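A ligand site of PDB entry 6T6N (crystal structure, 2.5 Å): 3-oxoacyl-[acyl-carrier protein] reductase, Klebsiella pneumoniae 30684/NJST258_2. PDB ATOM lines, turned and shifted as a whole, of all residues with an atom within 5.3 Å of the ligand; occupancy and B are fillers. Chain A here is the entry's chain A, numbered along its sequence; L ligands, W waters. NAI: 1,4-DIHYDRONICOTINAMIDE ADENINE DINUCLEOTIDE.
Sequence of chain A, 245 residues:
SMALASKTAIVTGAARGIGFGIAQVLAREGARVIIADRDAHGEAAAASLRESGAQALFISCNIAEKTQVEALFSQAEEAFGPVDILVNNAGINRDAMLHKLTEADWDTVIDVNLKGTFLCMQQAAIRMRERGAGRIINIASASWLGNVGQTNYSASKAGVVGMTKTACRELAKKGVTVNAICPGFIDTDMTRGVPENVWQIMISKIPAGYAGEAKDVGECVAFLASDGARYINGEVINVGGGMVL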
ATOM      1  N   GLY A  13      -7.580   3.506 -20.923  1.00  0.00           N
ATOM      2  CA  GLY A  13      -7.982   2.135 -21.241  1.00  0.00           C
ATOM      3  C   GLY A  13      -7.745   1.160 -20.110  1.00  0.00           C
ATOM      4  O   GLY A  13      -7.538  -0.045 -20.340  1.00  0.00           O
ATOM      5  N   ALA A  14      -7.776   1.668 -18.879  1.00  0.00           N
ATOM      6  CA  ALA A  14      -7.391   0.887 -17.698  1.00  0.00           C
ATOM      7  C   ALA A  14      -8.547   0.159 -16.986  1.00  0.00           C
ATOM      8  O   ALA A  14      -8.355  -0.385 -15.898  1.00  0.00           O
ATOM      9  CB  ALA A  14      -6.620   1.772 -16.740  1.00  0.00           C
ATOM     10  N   ALA A  15      -9.729   0.136 -17.607  1.00  0.00           N
ATOM     11  CA  ALA A  15     -10.852  -0.661 -17.075  1.00  0.00           C
ATOM     12  C   ALA A  15     -10.582  -2.153 -17.061  1.00  0.00           C
ATOM     13  O   ALA A  15     -11.073  -2.854 -16.186  1.00  0.00           O
ATOM     14  CB  ALA A  15     -12.130  -0.375 -17.865  1.00  0.00           C
ATOM     15  N   ARG A  16      -9.821  -2.638 -18.042  1.00  0.00           N
ATOM     16  CA  ARG A  16      -9.493  -4.061 -18.147  1.00  0.00           C
ATOM     17  C   ARG A  16      -8.177  -4.286 -18.914  1.00  0.00           C
ATOM     18  O   ARG A  16      -7.555  -3.329 -19.376  1.00  0.00           O
ATOM     19  CB  ARG A  16     -10.644  -4.821 -18.842  1.00  0.00           C
ATOM     20  CG  ARG A  16     -10.793  -4.569 -20.323  1.00  0.00           C
ATOM     21  CD  ARG A  16     -12.122  -5.151 -20.800  1.00  0.00           C
ATOM     22  NE  ARG A  16     -12.358  -4.919 -22.209  1.00  0.00           N
ATOM     23  CZ  ARG A  16     -13.335  -4.171 -22.751  1.00  0.00           C
ATOM     24  NH1 ARG A  16     -14.248  -3.523 -22.013  1.00  0.00           N
ATOM     25  NH2 ARG A  16     -13.403  -4.065 -24.082  1.00  0.00           N
ATOM     26  N   GLY A  17      -7.771  -5.547 -18.998  1.00  0.00           N
ATOM     27  CA  GLY A  17      -6.656  -5.962 -19.842  1.00  0.00           C
ATOM     28  C   GLY A  17      -5.314  -5.360 -19.417  1.00  0.00           C
ATOM     29  O   GLY A  17      -5.032  -5.201 -18.232  1.00  0.00           O
ATOM     30  N   ILE A  18      -4.525  -4.996 -20.426  1.00  0.00           N
ATOM     31  CA  ILE A  18      -3.173  -4.475 -20.198  1.00  0.00           C
ATOM     32  C   ILE A  18      -3.228  -3.202 -19.364  1.00  0.00           C
ATOM     33  O   ILE A  18      -2.461  -3.053 -18.417  1.00  0.00           O
ATOM     34  CB  ILE A  18      -2.427  -4.236 -21.534  1.00  0.00           C
ATOM     35  CG1 ILE A  18      -2.091  -5.606 -22.168  1.00  0.00           C
ATOM     36  CG2 ILE A  18      -1.125  -3.459 -21.308  1.00  0.00           C
ATOM     37  CD1 ILE A  18      -1.687  -5.521 -23.630  1.00  0.00           C
ATOM     38  N   GLY A  19      -4.130  -2.302 -19.719  1.00  0.00           N
ATOM     39  CA  GLY A  19      -4.288  -1.064 -18.969  1.00  0.00           C
ATOM     40  C   GLY A  19      -4.520  -1.274 -17.482  1.00  0.00           C
ATOM     41  O   GLY A  19      -3.923  -0.588 -16.640  1.00  0.00           O
ATOM     42  N   ALA A  36      -8.711   6.081 -16.688  1.00  0.00           N
ATOM     43  CA  ALA A  36      -9.438   6.801 -17.724  1.00  0.00           C
ATOM     44  C   ALA A  36      -9.910   5.794 -18.755  1.00  0.00           C
ATOM     45  O   ALA A  36      -9.090   5.067 -19.304  1.00  0.00           O
ATOM     46  CB  ALA A  36      -8.563   7.851 -18.363  1.00  0.00           C
ATOM     47  N   ASP A  37     -11.212   5.736 -18.993  1.00  0.00           N
ATOM     48  CA  ASP A  37     -11.784   4.746 -19.909  1.00  0.00           C
ATOM     49  C   ASP A  37     -13.133   5.210 -20.405  1.00  0.00           C
ATOM     50  O   ASP A  37     -13.786   6.019 -19.749  1.00  0.00           O
ATOM     51  CB  ASP A  37     -11.916   3.384 -19.214  1.00  0.00           C
ATOM     52  CG  ASP A  37     -11.902   2.216 -20.197  1.00  0.00           C
ATOM     53  OD1 ASP A  37     -12.833   2.113 -21.017  1.00  0.00           O
ATOM     54  OD2 ASP A  37     -10.955   1.391 -20.134  1.00  0.00           O
ATOM     55  N   ARG A  38     -13.546   4.736 -21.572  1.00  0.00           N
ATOM     56  CA  ARG A  38     -14.868   5.059 -22.112  1.00  0.00           C
ATOM     57  C   ARG A  38     -15.969   4.201 -21.470  1.00  0.00           C
ATOM     58  O   ARG A  38     -17.144   4.565 -21.484  1.00  0.00           O
ATOM     59  CB  ARG A  38     -14.908   4.965 -23.635  1.00  0.00           C
ATOM     60  CG  ARG A  38     -14.881   3.545 -24.205  1.00  0.00           C
ATOM     61  CD  ARG A  38     -14.951   3.565 -25.730  1.00  0.00           C
ATOM     62  NE  ARG A  38     -16.140   4.263 -26.193  1.00  0.00           N
ATOM     63  CZ  ARG A  38     -16.289   4.870 -27.365  1.00  0.00           C
ATOM     64  NH1 ARG A  38     -15.328   4.873 -28.287  1.00  0.00           N
ATOM     65  NH2 ARG A  38     -17.440   5.481 -27.612  1.00  0.00           N
ATOM     66  N   ASP A  39     -15.584   3.050 -20.907  1.00  0.00           N
ATOM     67  CA  ASP A  39     -16.499   2.088 -20.325  1.00  0.00           C
ATOM     68  C   ASP A  39     -16.636   2.252 -18.804  1.00  0.00           C
ATOM     69  O   ASP A  39     -15.642   2.400 -18.087  1.00  0.00           O
ATOM     70  CB  ASP A  39     -16.003   0.702 -20.647  1.00  0.00           C
ATOM     71  CG  ASP A  39     -16.947  -0.389 -20.250  1.00  0.00           C
ATOM     72  OD1 ASP A  39     -18.167  -0.216 -20.055  1.00  0.00           O
ATOM     73  OD2 ASP A  39     -16.383  -1.444 -20.043  1.00  0.00           O
ATOM     74  N   CYS A  61     -14.081   8.866 -20.080  1.00  0.00           N
ATOM     75  CA  CYS A  61     -13.415   9.620 -21.139  1.00  0.00           C
ATOM     76  C   CYS A  61     -13.317   8.809 -22.424  1.00  0.00           C
ATOM     77  O   CYS A  61     -12.832   7.669 -22.402  1.00  0.00           O
ATOM     78  CB  CYS A  61     -12.021  10.055 -20.718  1.00  0.00           C
ATOM     79  SG  CYS A  61     -11.193  11.088 -21.958  1.00  0.00           S
ATOM     80  N   ASN A  62     -13.738   9.415 -23.523  1.00  0.00           N
ATOM     81  CA  ASN A  62     -13.444   8.901 -24.847  1.00  0.00           C
ATOM     82  C   ASN A  62     -12.271   9.730 -25.377  1.00  0.00           C
ATOM     83  O   ASN A  62     -12.435  10.917 -25.688  1.00  0.00           O
ATOM     84  CB  ASN A  62     -14.659   9.011 -25.761  1.00  0.00           C
ATOM     85  CG  ASN A  62     -14.382   8.623 -27.194  1.00  0.00           C
ATOM     86  OD1 ASN A  62     -13.305   8.128 -27.526  1.00  0.00           O
ATOM     87  ND2 ASN A  62     -15.338   8.865 -28.058  1.00  0.00           N
ATOM     88  N   ILE A  63     -11.104   9.092 -25.507  1.00  0.00           N
ATOM     89  CA  ILE A  63      -9.870   9.815 -25.863  1.00  0.00           C
ATOM     90  C   ILE A  63      -9.892  10.444 -27.255  1.00  0.00           C
ATOM     91  O   ILE A  63      -9.107  11.357 -27.527  1.00  0.00           O
ATOM     92  CB  ILE A  63      -8.596   8.965 -25.684  1.00  0.00           C
ATOM     93  CG1 ILE A  63      -8.588   7.730 -26.603  1.00  0.00           C
ATOM     94  CG2 ILE A  63      -8.454   8.530 -24.225  1.00  0.00           C
ATOM     95  CD1 ILE A  63      -7.212   7.131 -26.772  1.00  0.00           C
ATOM     96  N   ALA A  64     -10.783   9.972 -28.124  1.00  0.00           N
ATOM     97  CA  ALA A  64     -10.972  10.564 -29.456  1.00  0.00           C
ATOM     98  C   ALA A  64     -11.616  11.963 -29.471  1.00  0.00           C
ATOM     99  O   ALA A  64     -11.600  12.629 -30.508  1.00  0.00           O
ATOM    100  CB  ALA A  64     -11.793   9.618 -30.318  1.00  0.00           C
ATOM    101  N   ASN A  89      -2.651   3.791 -23.203  1.00  0.00           N
ATOM    102  CA  ASN A  89      -2.891   2.374 -23.458  1.00  0.00           C
ATOM    103  C   ASN A  89      -4.178   2.102 -24.267  1.00  0.00           C
ATOM    104  O   ASN A  89      -4.258   1.105 -24.981  1.00  0.00           O
ATOM    105  CB  ASN A  89      -2.866   1.615 -22.123  1.00  0.00           C
ATOM    106  CG  ASN A  89      -3.484   0.240 -22.205  1.00  0.00           C
ATOM    107  OD1 ASN A  89      -2.813  -0.730 -22.548  1.00  0.00           O
ATOM    108  ND2 ASN A  89      -4.778   0.142 -21.884  1.00  0.00           N
ATOM    109  N   ALA A  90      -5.170   2.982 -24.169  1.00  0.00           N
ATOM    110  CA  ALA A  90      -6.447   2.743 -24.859  1.00  0.00           C
ATOM    111  C   ALA A  90      -6.252   2.494 -26.338  1.00  0.00           C
ATOM    112  O   ALA A  90      -5.501   3.204 -26.976  1.00  0.00           O
ATOM    113  CB  ALA A  90      -7.403   3.907 -24.654  1.00  0.00           C
ATOM    114  N   GLY A  91      -6.908   1.450 -26.841  1.00  0.00           N
ATOM    115  CA  GLY A  91      -6.903   1.176 -28.274  1.00  0.00           C
ATOM    116  C   GLY A  91      -7.883   0.098 -28.675  1.00  0.00           C
ATOM    117  O   GLY A  91      -8.378  -0.644 -27.828  1.00  0.00           O
ATOM    118  N   ILE A  92      -8.157   0.021 -29.974  1.00  0.00           N
ATOM    119  CA  ILE A  92      -9.100  -0.933 -30.520  1.00  0.00           C
ATOM    120  C   ILE A  92      -8.558  -1.574 -31.799  1.00  0.00           C
ATOM    121  O   ILE A  92      -7.650  -1.036 -32.427  1.00  0.00           O
ATOM    122  CB  ILE A  92     -10.460  -0.265 -30.848  1.00  0.00           C
ATOM    123  CG1 ILE A  92     -10.258   0.957 -31.756  1.00  0.00           C
ATOM    124  CG2 ILE A  92     -11.178   0.092 -29.554  1.00  0.00           C
ATOM    125  CD1 ILE A  92     -11.531   1.493 -32.353  1.00  0.00           C
ATOM    126  N   ASN A  93      -9.146  -2.715 -32.150  1.00  0.00           N
ATOM    127  CA  ASN A  93      -8.923  -3.362 -33.448  1.00  0.00           C
ATOM    128  C   ASN A  93     -10.218  -3.399 -34.242  1.00  0.00           C
ATOM    129  O   ASN A  93     -11.279  -3.653 -33.687  1.00  0.00           O
ATOM    130  CB  ASN A  93      -8.440  -4.798 -33.260  1.00  0.00           C
ATOM    131  CG  ASN A  93      -6.973  -4.868 -32.881  1.00  0.00           C
ATOM    132  OD1 ASN A  93      -6.110  -5.122 -33.730  1.00  0.00           O
ATOM    133  ND2 ASN A  93      -6.688  -4.640 -31.609  1.00  0.00           N
ATOM    134  N   VAL A 112      -9.249   6.590 -32.620  1.00  0.00           N
ATOM    135  CA  VAL A 112      -8.966   6.195 -31.234  1.00  0.00           C
ATOM    136  C   VAL A 112      -7.464   6.030 -30.998  1.00  0.00           C
ATOM    137  O   VAL A 112      -6.894   6.682 -30.123  1.00  0.00           O
ATOM    138  CB  VAL A 112      -9.705   4.878 -30.851  1.00  0.00           C
ATOM    139  CG1 VAL A 112      -9.396   4.458 -29.423  1.00  0.00           C
ATOM    140  CG2 VAL A 112     -11.213   5.063 -30.997  1.00  0.00           C
ATOM    141  N   ASN A 113      -6.835   5.150 -31.765  1.00  0.00           N
ATOM    142  CA  ASN A 113      -5.454   4.730 -31.492  1.00  0.00           C
ATOM    143  C   ASN A 113      -4.440   5.824 -31.760  1.00  0.00           C
ATOM    144  O   ASN A 113      -3.462   5.966 -31.018  1.00  0.00           O
ATOM    145  CB  ASN A 113      -5.081   3.510 -32.339  1.00  0.00           C
ATOM    146  CG  ASN A 113      -5.880   2.267 -31.989  1.00  0.00           C
ATOM    147  OD1 ASN A 113      -6.787   2.300 -31.157  1.00  0.00           O
ATOM    148  ND2 ASN A 113      -5.544   1.161 -32.625  1.00  0.00           N
ATOM    149  N   ILE A 139       1.554   2.816 -25.420  1.00  0.00           N
ATOM    150  CA  ILE A 139       1.477   1.404 -25.708  1.00  0.00           C
ATOM    151  C   ILE A 139       1.205   1.305 -27.200  1.00  0.00           C
ATOM    152  O   ILE A 139       0.156   1.708 -27.683  1.00  0.00           O
ATOM    153  CB  ILE A 139       0.357   0.710 -24.903  1.00  0.00           C
ATOM    154  CG1 ILE A 139       0.547   0.956 -23.403  1.00  0.00           C
ATOM    155  CG2 ILE A 139       0.333  -0.793 -25.191  1.00  0.00           C
ATOM    156  CD1 ILE A 139       1.911   0.536 -22.851  1.00  0.00           C
ATOM    157  N   ALA A 140       2.198   0.807 -27.931  1.00  0.00           N
ATOM    158  CA  ALA A 140       2.071   0.616 -29.355  1.00  0.00           C
ATOM    159  C   ALA A 140       1.664  -0.848 -29.573  1.00  0.00           C
ATOM    160  O   ALA A 140       0.723  -1.305 -28.942  1.00  0.00           O
ATOM    161  CB  ALA A 140       3.366   1.012 -30.041  1.00  0.00           C
ATOM    162  N   SER A 141       2.394  -1.592 -30.417  1.00  0.00           N
ATOM    163  CA  SER A 141       2.118  -2.991 -30.701  1.00  0.00           C
ATOM    164  C   SER A 141       3.233  -3.513 -31.575  1.00  0.00           C
ATOM    165  O   SER A 141       3.807  -2.767 -32.368  1.00  0.00           O
ATOM    166  CB  SER A 141       0.809  -3.143 -31.491  1.00  0.00           C
ATOM    167  OG  SER A 141       0.675  -4.458 -32.030  1.00  0.00           O
ATOM    168  N   ALA A 142       3.487  -4.806 -31.466  1.00  0.00           N
ATOM    169  CA  ALA A 142       4.374  -5.506 -32.407  1.00  0.00           C
ATOM    170  C   ALA A 142       3.914  -5.377 -33.869  1.00  0.00           C
ATOM    171  O   ALA A 142       4.715  -5.554 -34.793  1.00  0.00           O
ATOM    172  CB  ALA A 142       4.448  -6.965 -32.017  1.00  0.00           C
ATOM    173  N   TYR A 153      -4.728  -0.859 -38.081  1.00  0.00           N
ATOM    174  CA  TYR A 153      -4.100  -0.989 -36.759  1.00  0.00           C
ATOM    175  C   TYR A 153      -2.587  -0.721 -36.834  1.00  0.00           C
ATOM    176  O   TYR A 153      -2.060   0.032 -36.013  1.00  0.00           O
ATOM    177  CB  TYR A 153      -4.363  -2.381 -36.203  1.00  0.00           C
ATOM    178  CG  TYR A 153      -3.931  -2.616 -34.785  1.00  0.00           C
ATOM    179  CD1 TYR A 153      -4.624  -2.058 -33.702  1.00  0.00           C
ATOM    180  CD2 TYR A 153      -2.841  -3.443 -34.509  1.00  0.00           C
ATOM    181  CE1 TYR A 153      -4.230  -2.312 -32.403  1.00  0.00           C
ATOM    182  CE2 TYR A 153      -2.441  -3.711 -33.204  1.00  0.00           C
ATOM    183  CZ  TYR A 153      -3.133  -3.152 -32.153  1.00  0.00           C
ATOM    184  OH  TYR A 153      -2.708  -3.430 -30.867  1.00  0.00           O
ATOM    185  N   LYS A 157      -0.524   2.279 -34.962  1.00  0.00           N
ATOM    186  CA  LYS A 157       0.501   2.008 -33.964  1.00  0.00           C
ATOM    187  C   LYS A 157       1.899   2.463 -34.404  1.00  0.00           C
ATOM    188  O   LYS A 157       2.667   2.916 -33.568  1.00  0.00           O
ATOM    189  CB  LYS A 157       0.503   0.528 -33.591  1.00  0.00           C
ATOM    190  CG  LYS A 157      -0.785   0.051 -32.911  1.00  0.00           C
ATOM    191  CD  LYS A 157      -1.089   0.814 -31.632  1.00  0.00           C
ATOM    192  CE  LYS A 157      -2.043   0.016 -30.745  1.00  0.00           C
ATOM    193  NZ  LYS A 157      -2.156   0.585 -29.365  1.00  0.00           N
ATOM    194  N   PRO A 183       3.846  -4.347 -26.759  1.00  0.00           N
ATOM    195  CA  PRO A 183       3.578  -5.699 -26.268  1.00  0.00           C
ATOM    196  C   PRO A 183       3.555  -6.672 -27.435  1.00  0.00           C
ATOM    197  O   PRO A 183       3.156  -6.284 -28.559  1.00  0.00           O
ATOM    198  CB  PRO A 183       2.168  -5.575 -25.673  1.00  0.00           C
ATOM    199  CG  PRO A 183       1.968  -4.120 -25.440  1.00  0.00           C
ATOM    200  CD  PRO A 183       2.673  -3.466 -26.592  1.00  0.00           C
ATOM    201  N   GLY A 184       4.025  -7.885 -27.201  1.00  0.00           N
ATOM    202  CA  GLY A 184       3.986  -8.937 -28.221  1.00  0.00           C
ATOM    203  C   GLY A 184       2.645  -9.634 -28.200  1.00  0.00           C
ATOM    204  O   GLY A 184       1.689  -9.095 -28.714  1.00  0.00           O
ATOM    205  N   PHE A 185       2.587 -10.844 -27.644  1.00  0.00           N
ATOM    206  CA  PHE A 185       1.352 -11.619 -27.519  1.00  0.00           C
ATOM    207  C   PHE A 185       1.069 -11.697 -25.983  1.00  0.00           C
ATOM    208  O   PHE A 185       1.776 -12.400 -25.254  1.00  0.00           O
ATOM    209  CB  PHE A 185       1.496 -13.004 -28.093  1.00  0.00           C
ATOM    210  CG  PHE A 185       1.276 -13.149 -29.577  1.00  0.00           C
ATOM    211  CD1 PHE A 185       0.197 -12.588 -30.243  1.00  0.00           C
ATOM    212  CD2 PHE A 185       2.123 -13.979 -30.279  1.00  0.00           C
ATOM    213  CE1 PHE A 185       0.032 -12.777 -31.613  1.00  0.00           C
ATOM    214  CE2 PHE A 185       2.044 -14.094 -31.690  1.00  0.00           C
ATOM    215  CZ  PHE A 185       0.953 -13.551 -32.335  1.00  0.00           C
ATOM    216  N   ILE A 186       0.054 -10.973 -25.530  1.00  0.00           N
ATOM    217  CA  ILE A 186      -0.295 -10.880 -24.133  1.00  0.00           C
ATOM    218  C   ILE A 186      -1.666 -11.524 -23.873  1.00  0.00           C
ATOM    219  O   ILE A 186      -2.627 -11.289 -24.611  1.00  0.00           O
ATOM    220  CB  ILE A 186      -0.375  -9.409 -23.645  1.00  0.00           C
ATOM    221  CG1 ILE A 186       0.912  -8.646 -23.965  1.00  0.00           C
ATOM    222  CG2 ILE A 186      -0.636  -9.342 -22.129  1.00  0.00           C
ATOM    223  CD1 ILE A 186       2.189  -9.196 -23.340  1.00  0.00           C
ATOM    224  N   THR A 188      -4.994 -11.603 -22.513  1.00  0.00           N
ATOM    225  CA  THR A 188      -6.106 -10.721 -22.109  1.00  0.00           C
ATOM    226  C   THR A 188      -7.428 -11.304 -22.630  1.00  0.00           C
ATOM    227  O   THR A 188      -7.412 -12.362 -23.256  1.00  0.00           O
ATOM    228  CB  THR A 188      -5.943  -9.272 -22.660  1.00  0.00           C
ATOM    229  OG1 THR A 188      -5.986  -9.281 -24.103  1.00  0.00           O
ATOM    230  CG2 THR A 188      -4.639  -8.646 -22.178  1.00  0.00           C
ATOM    231  N   ASP A 189      -8.535 -10.611 -22.400  1.00  0.00           N
ATOM    232  CA  ASP A 189      -9.847 -10.999 -22.940  1.00  0.00           C
ATOM    233  C   ASP A 189      -9.859 -11.093 -24.481  1.00  0.00           C
ATOM    234  O   ASP A 189     -10.441 -12.036 -25.028  1.00  0.00           O
ATOM    235  CB  ASP A 189     -10.963 -10.041 -22.478  1.00  0.00           C
ATOM    236  CG  ASP A 189     -11.140 -10.025 -20.953  1.00  0.00           C
ATOM    237  OD1 ASP A 189     -10.904 -11.079 -20.310  1.00  0.00           O
ATOM    238  OD2 ASP A 189     -11.522  -8.959 -20.396  1.00  0.00           O
ATOM    239  N   MET A 190      -9.192 -10.142 -25.167  1.00  0.00           N
ATOM    240  CA  MET A 190      -9.107 -10.153 -26.634  1.00  0.00           C
ATOM    241  C   MET A 190      -8.376 -11.367 -27.219  1.00  0.00           C
ATOM    242  O   MET A 190      -8.821 -11.947 -28.219  1.00  0.00           O
ATOM    243  CB  MET A 190      -8.456  -8.854 -27.145  1.00  0.00           C
ATOM    244  CG  MET A 190      -9.351  -7.603 -27.004  1.00  0.00           C
ATOM    245  SD  MET A 190     -10.948  -7.560 -27.911  1.00  0.00           S
ATOM    246  CE  MET A 190     -10.464  -7.178 -29.613  1.00  0.00           C
ATOM    247  N   THR A 191      -7.280 -11.757 -26.589  1.00  0.00           N
ATOM    248  CA  THR A 191      -6.476 -12.901 -27.054  1.00  0.00           C
ATOM    249  C   THR A 191      -7.000 -14.257 -26.567  1.00  0.00           C
ATOM    250  O   THR A 191      -6.726 -15.278 -27.224  1.00  0.00           O
ATOM    251  CB  THR A 191      -5.001 -12.758 -26.626  1.00  0.00           C
ATOM    252  OG1 THR A 191      -4.919 -12.567 -25.201  1.00  0.00           O
ATOM    253  CG2 THR A 191      -4.360 -11.575 -27.313  1.00  0.00           C
HETATM  254  PA  NAI L   1      -8.821  -4.380 -24.328  1.00  0.00           P
HETATM  255  O1A NAI L   1      -9.659  -4.290 -25.579  1.00  0.00           O
HETATM  256  O2A NAI L   1      -8.881  -5.603 -23.405  1.00  0.00           O
HETATM  257  O5B NAI L   1      -9.016  -3.047 -23.444  1.00  0.00           O
HETATM  258  C5B NAI L   1      -8.891  -1.756 -24.004  1.00  0.00           C
HETATM  259  C4B NAI L   1      -9.555  -0.738 -23.084  1.00  0.00           C
HETATM  260  O4B NAI L   1      -9.468   0.521 -23.744  1.00  0.00           O
HETATM  261  C3B NAI L   1     -11.038  -1.013 -22.787  1.00  0.00           C
HETATM  262  O3B NAI L   1     -11.329  -0.837 -21.391  1.00  0.00           O
HETATM  263  C2B NAI L   1     -11.777  -0.011 -23.651  1.00  0.00           C
HETATM  264  O2B NAI L   1     -13.024   0.438 -23.093  1.00  0.00           O
HETATM  265  C1B NAI L   1     -10.770   1.118 -23.722  1.00  0.00           C
HETATM  266  N9A NAI L   1     -11.038   2.041 -24.844  1.00  0.00           N
HETATM  267  C8A NAI L   1     -11.348   1.736 -26.123  1.00  0.00           C
HETATM  268  N7A NAI L   1     -11.558   2.860 -26.844  1.00  0.00           N
HETATM  269  C5A NAI L   1     -11.405   3.905 -26.015  1.00  0.00           C
HETATM  270  C6A NAI L   1     -11.495   5.365 -26.126  1.00  0.00           C
HETATM  271  N6A NAI L   1     -11.802   5.891 -27.323  1.00  0.00           N
HETATM  272  N1A NAI L   1     -11.244   6.127 -25.028  1.00  0.00           N
HETATM  273  C2A NAI L   1     -10.954   5.564 -23.834  1.00  0.00           C
HETATM  274  N3A NAI L   1     -10.859   4.231 -23.669  1.00  0.00           N
HETATM  275  C4A NAI L   1     -11.072   3.370 -24.700  1.00  0.00           C
HETATM  276  O3  NAI L   1      -7.302  -4.161 -24.876  1.00  0.00           O
HETATM  277  PN  NAI L   1      -5.948  -4.863 -24.333  1.00  0.00           P
HETATM  278  O1N NAI L   1      -5.854  -6.258 -24.905  1.00  0.00           O
HETATM  279  O2N NAI L   1      -5.785  -4.682 -22.826  1.00  0.00           O
HETATM  280  O5D NAI L   1      -4.981  -3.804 -25.079  1.00  0.00           O
HETATM  281  C5D NAI L   1      -4.492  -2.578 -24.496  1.00  0.00           C
HETATM  282  C4D NAI L   1      -3.570  -1.859 -25.473  1.00  0.00           C
HETATM  283  O4D NAI L   1      -2.479  -2.687 -25.872  1.00  0.00           O
HETATM  284  C3D NAI L   1      -4.289  -1.511 -26.771  1.00  0.00           C
HETATM  285  O3D NAI L   1      -3.764  -0.296 -27.306  1.00  0.00           O
HETATM  286  C2D NAI L   1      -3.989  -2.669 -27.703  1.00  0.00           C
HETATM  287  O2D NAI L   1      -4.198  -2.288 -29.059  1.00  0.00           O
HETATM  288  C1D NAI L   1      -2.543  -2.931 -27.280  1.00  0.00           C
HETATM  289  N1N NAI L   1      -2.026  -4.273 -27.599  1.00  0.00           N
HETATM  290  C2N NAI L   1      -2.577  -5.345 -27.052  1.00  0.00           C
HETATM  291  C3N NAI L   1      -2.100  -6.614 -27.347  1.00  0.00           C
HETATM  292  C7N NAI L   1      -2.722  -7.833 -26.755  1.00  0.00           C
HETATM  293  O7N NAI L   1      -2.075  -8.850 -26.880  1.00  0.00           O
HETATM  294  N7N NAI L   1      -3.935  -7.831 -26.164  1.00  0.00           N
HETATM  295  C4N NAI L   1      -0.945  -6.831 -28.290  1.00  0.00           C
HETATM  296  C5N NAI L   1      -0.431  -5.589 -28.827  1.00  0.00           C
HETATM  297  C6N NAI L   1      -0.984  -4.378 -28.448  1.00  0.00           C
HETATM  298  O   HOH W   1      -6.247  -2.322 -21.761  1.00  0.00           O
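An oxygen (O3B) of the ligand lies within hydrogen-bond range of the side-chain carboxylate (OD2) of Asp 37, at 2.6 Å.
The side-chain hydroxyl (OH) of Tyr 153 is in hydrogen-bond range of an oxygen (O2D) of the ligand, 2.6 Å away.
A nitrogen (N6A) of the ligand is in hydrogen-bond range of the side-chain amide oxygen (OD1) of Asn 62, 2.7 Å away.
The backbone NH (N) of Ile 18 is in hydrogen-bond range of an oxygen (O2N) of the ligand, 2.7 Å away.
An oxygen (O3D) of the ligand lies within hydrogen-bond range of the side-chain amino group of Lys 157, at 2.8 Å.
An oxygen (O3D) of the ligand lies within hydrogen-bond range of the backbone carbonyl oxygen (O) of Asn 89.
N1A of the ligand sits at hydrogen-bond distance from N of Ile 63, 3.0 Å away.
An oxygen (O1N) of the ligand lies within hydrogen-bond range of the side-chain hydroxyl (OG1) of Thr 188 (3.1 Å).
N of Ile 186 lies within hydrogen-bond range of O7N of the ligand (3.3 Å).
The backbone NH (N) of Arg 38 lies within hydrogen-bond range of a nitrogen (N3A) of the ligand, 3.4 Å away.
The guanidinium group (NE) of Arg 16 is in salt-bridge range of an oxygen (O2A) of the ligand, 3.7 Å away.
The side-chain carboxylate (OD1) of Asp 37 sits at hydrogen-bond distance from the backbone NH (N) of Asp 39, at 2.9 Å.
N of Ala 14 lies within hydrogen-bond range of OD2 of Asp 37, 3.4 Å away.
NZ of Lys 157 sits at hydrogen-bond distance from O of Ala 140.
The side-chain amide nitrogen (ND2) of Asn 89 lies close to the backbone NH (N) of Gly 19, at 3.3 Å.
The side-chain hydroxyl of Thr 188 lies close to the backbone NH of Met 190 (3.5 Å).
O of Cys 61 is in hydrogen-bond range of N of Arg 38 (3.1 Å).
O of Pro 183 is in hydrogen-bond range of N of Ala 142, 3.3 Å away.
The backbone NH of Ile 92 lies within hydrogen-bond range of the side-chain amide oxygen of Asn 113 (2.9 Å).
The backbone carbonyl oxygen (O) of Cys 61 sits close to a nitrogen (N1A) of the ligand (3.4 Å).
Merely in contact with the ligand: Gly 13, Ala 15, Gly 17, Asp 39, Ala 90, Gly 91, Ile 92, Val 112, Ile 139, Ala 140, Ser 141, Pro 183, Gly 184, Met 190 and Thr 191.
Hydrophobic or aromatic side chains that line the ligand: Ala 15, Ile 18, Ile 63, Ala 90, Ile 92, Val 112, Ile 139, Tyr 153, Ile 186 and Met 190.
Within 4 Å of the ligand: Gly 13, Ala 15, Arg 16, Gly 17, Ile 18, Asp 37, Arg 38, Asp 39, Cys 61, Asn 62, Ile 63, Asn 89, Ala 90, Gly 91, Ile 92, Val 112, Ile 139, Ala 140, Ser 141, Tyr 153, Lys 157, Pro 183, Gly 184, Ile 186, Thr 188, Met 190 and Thr 191.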
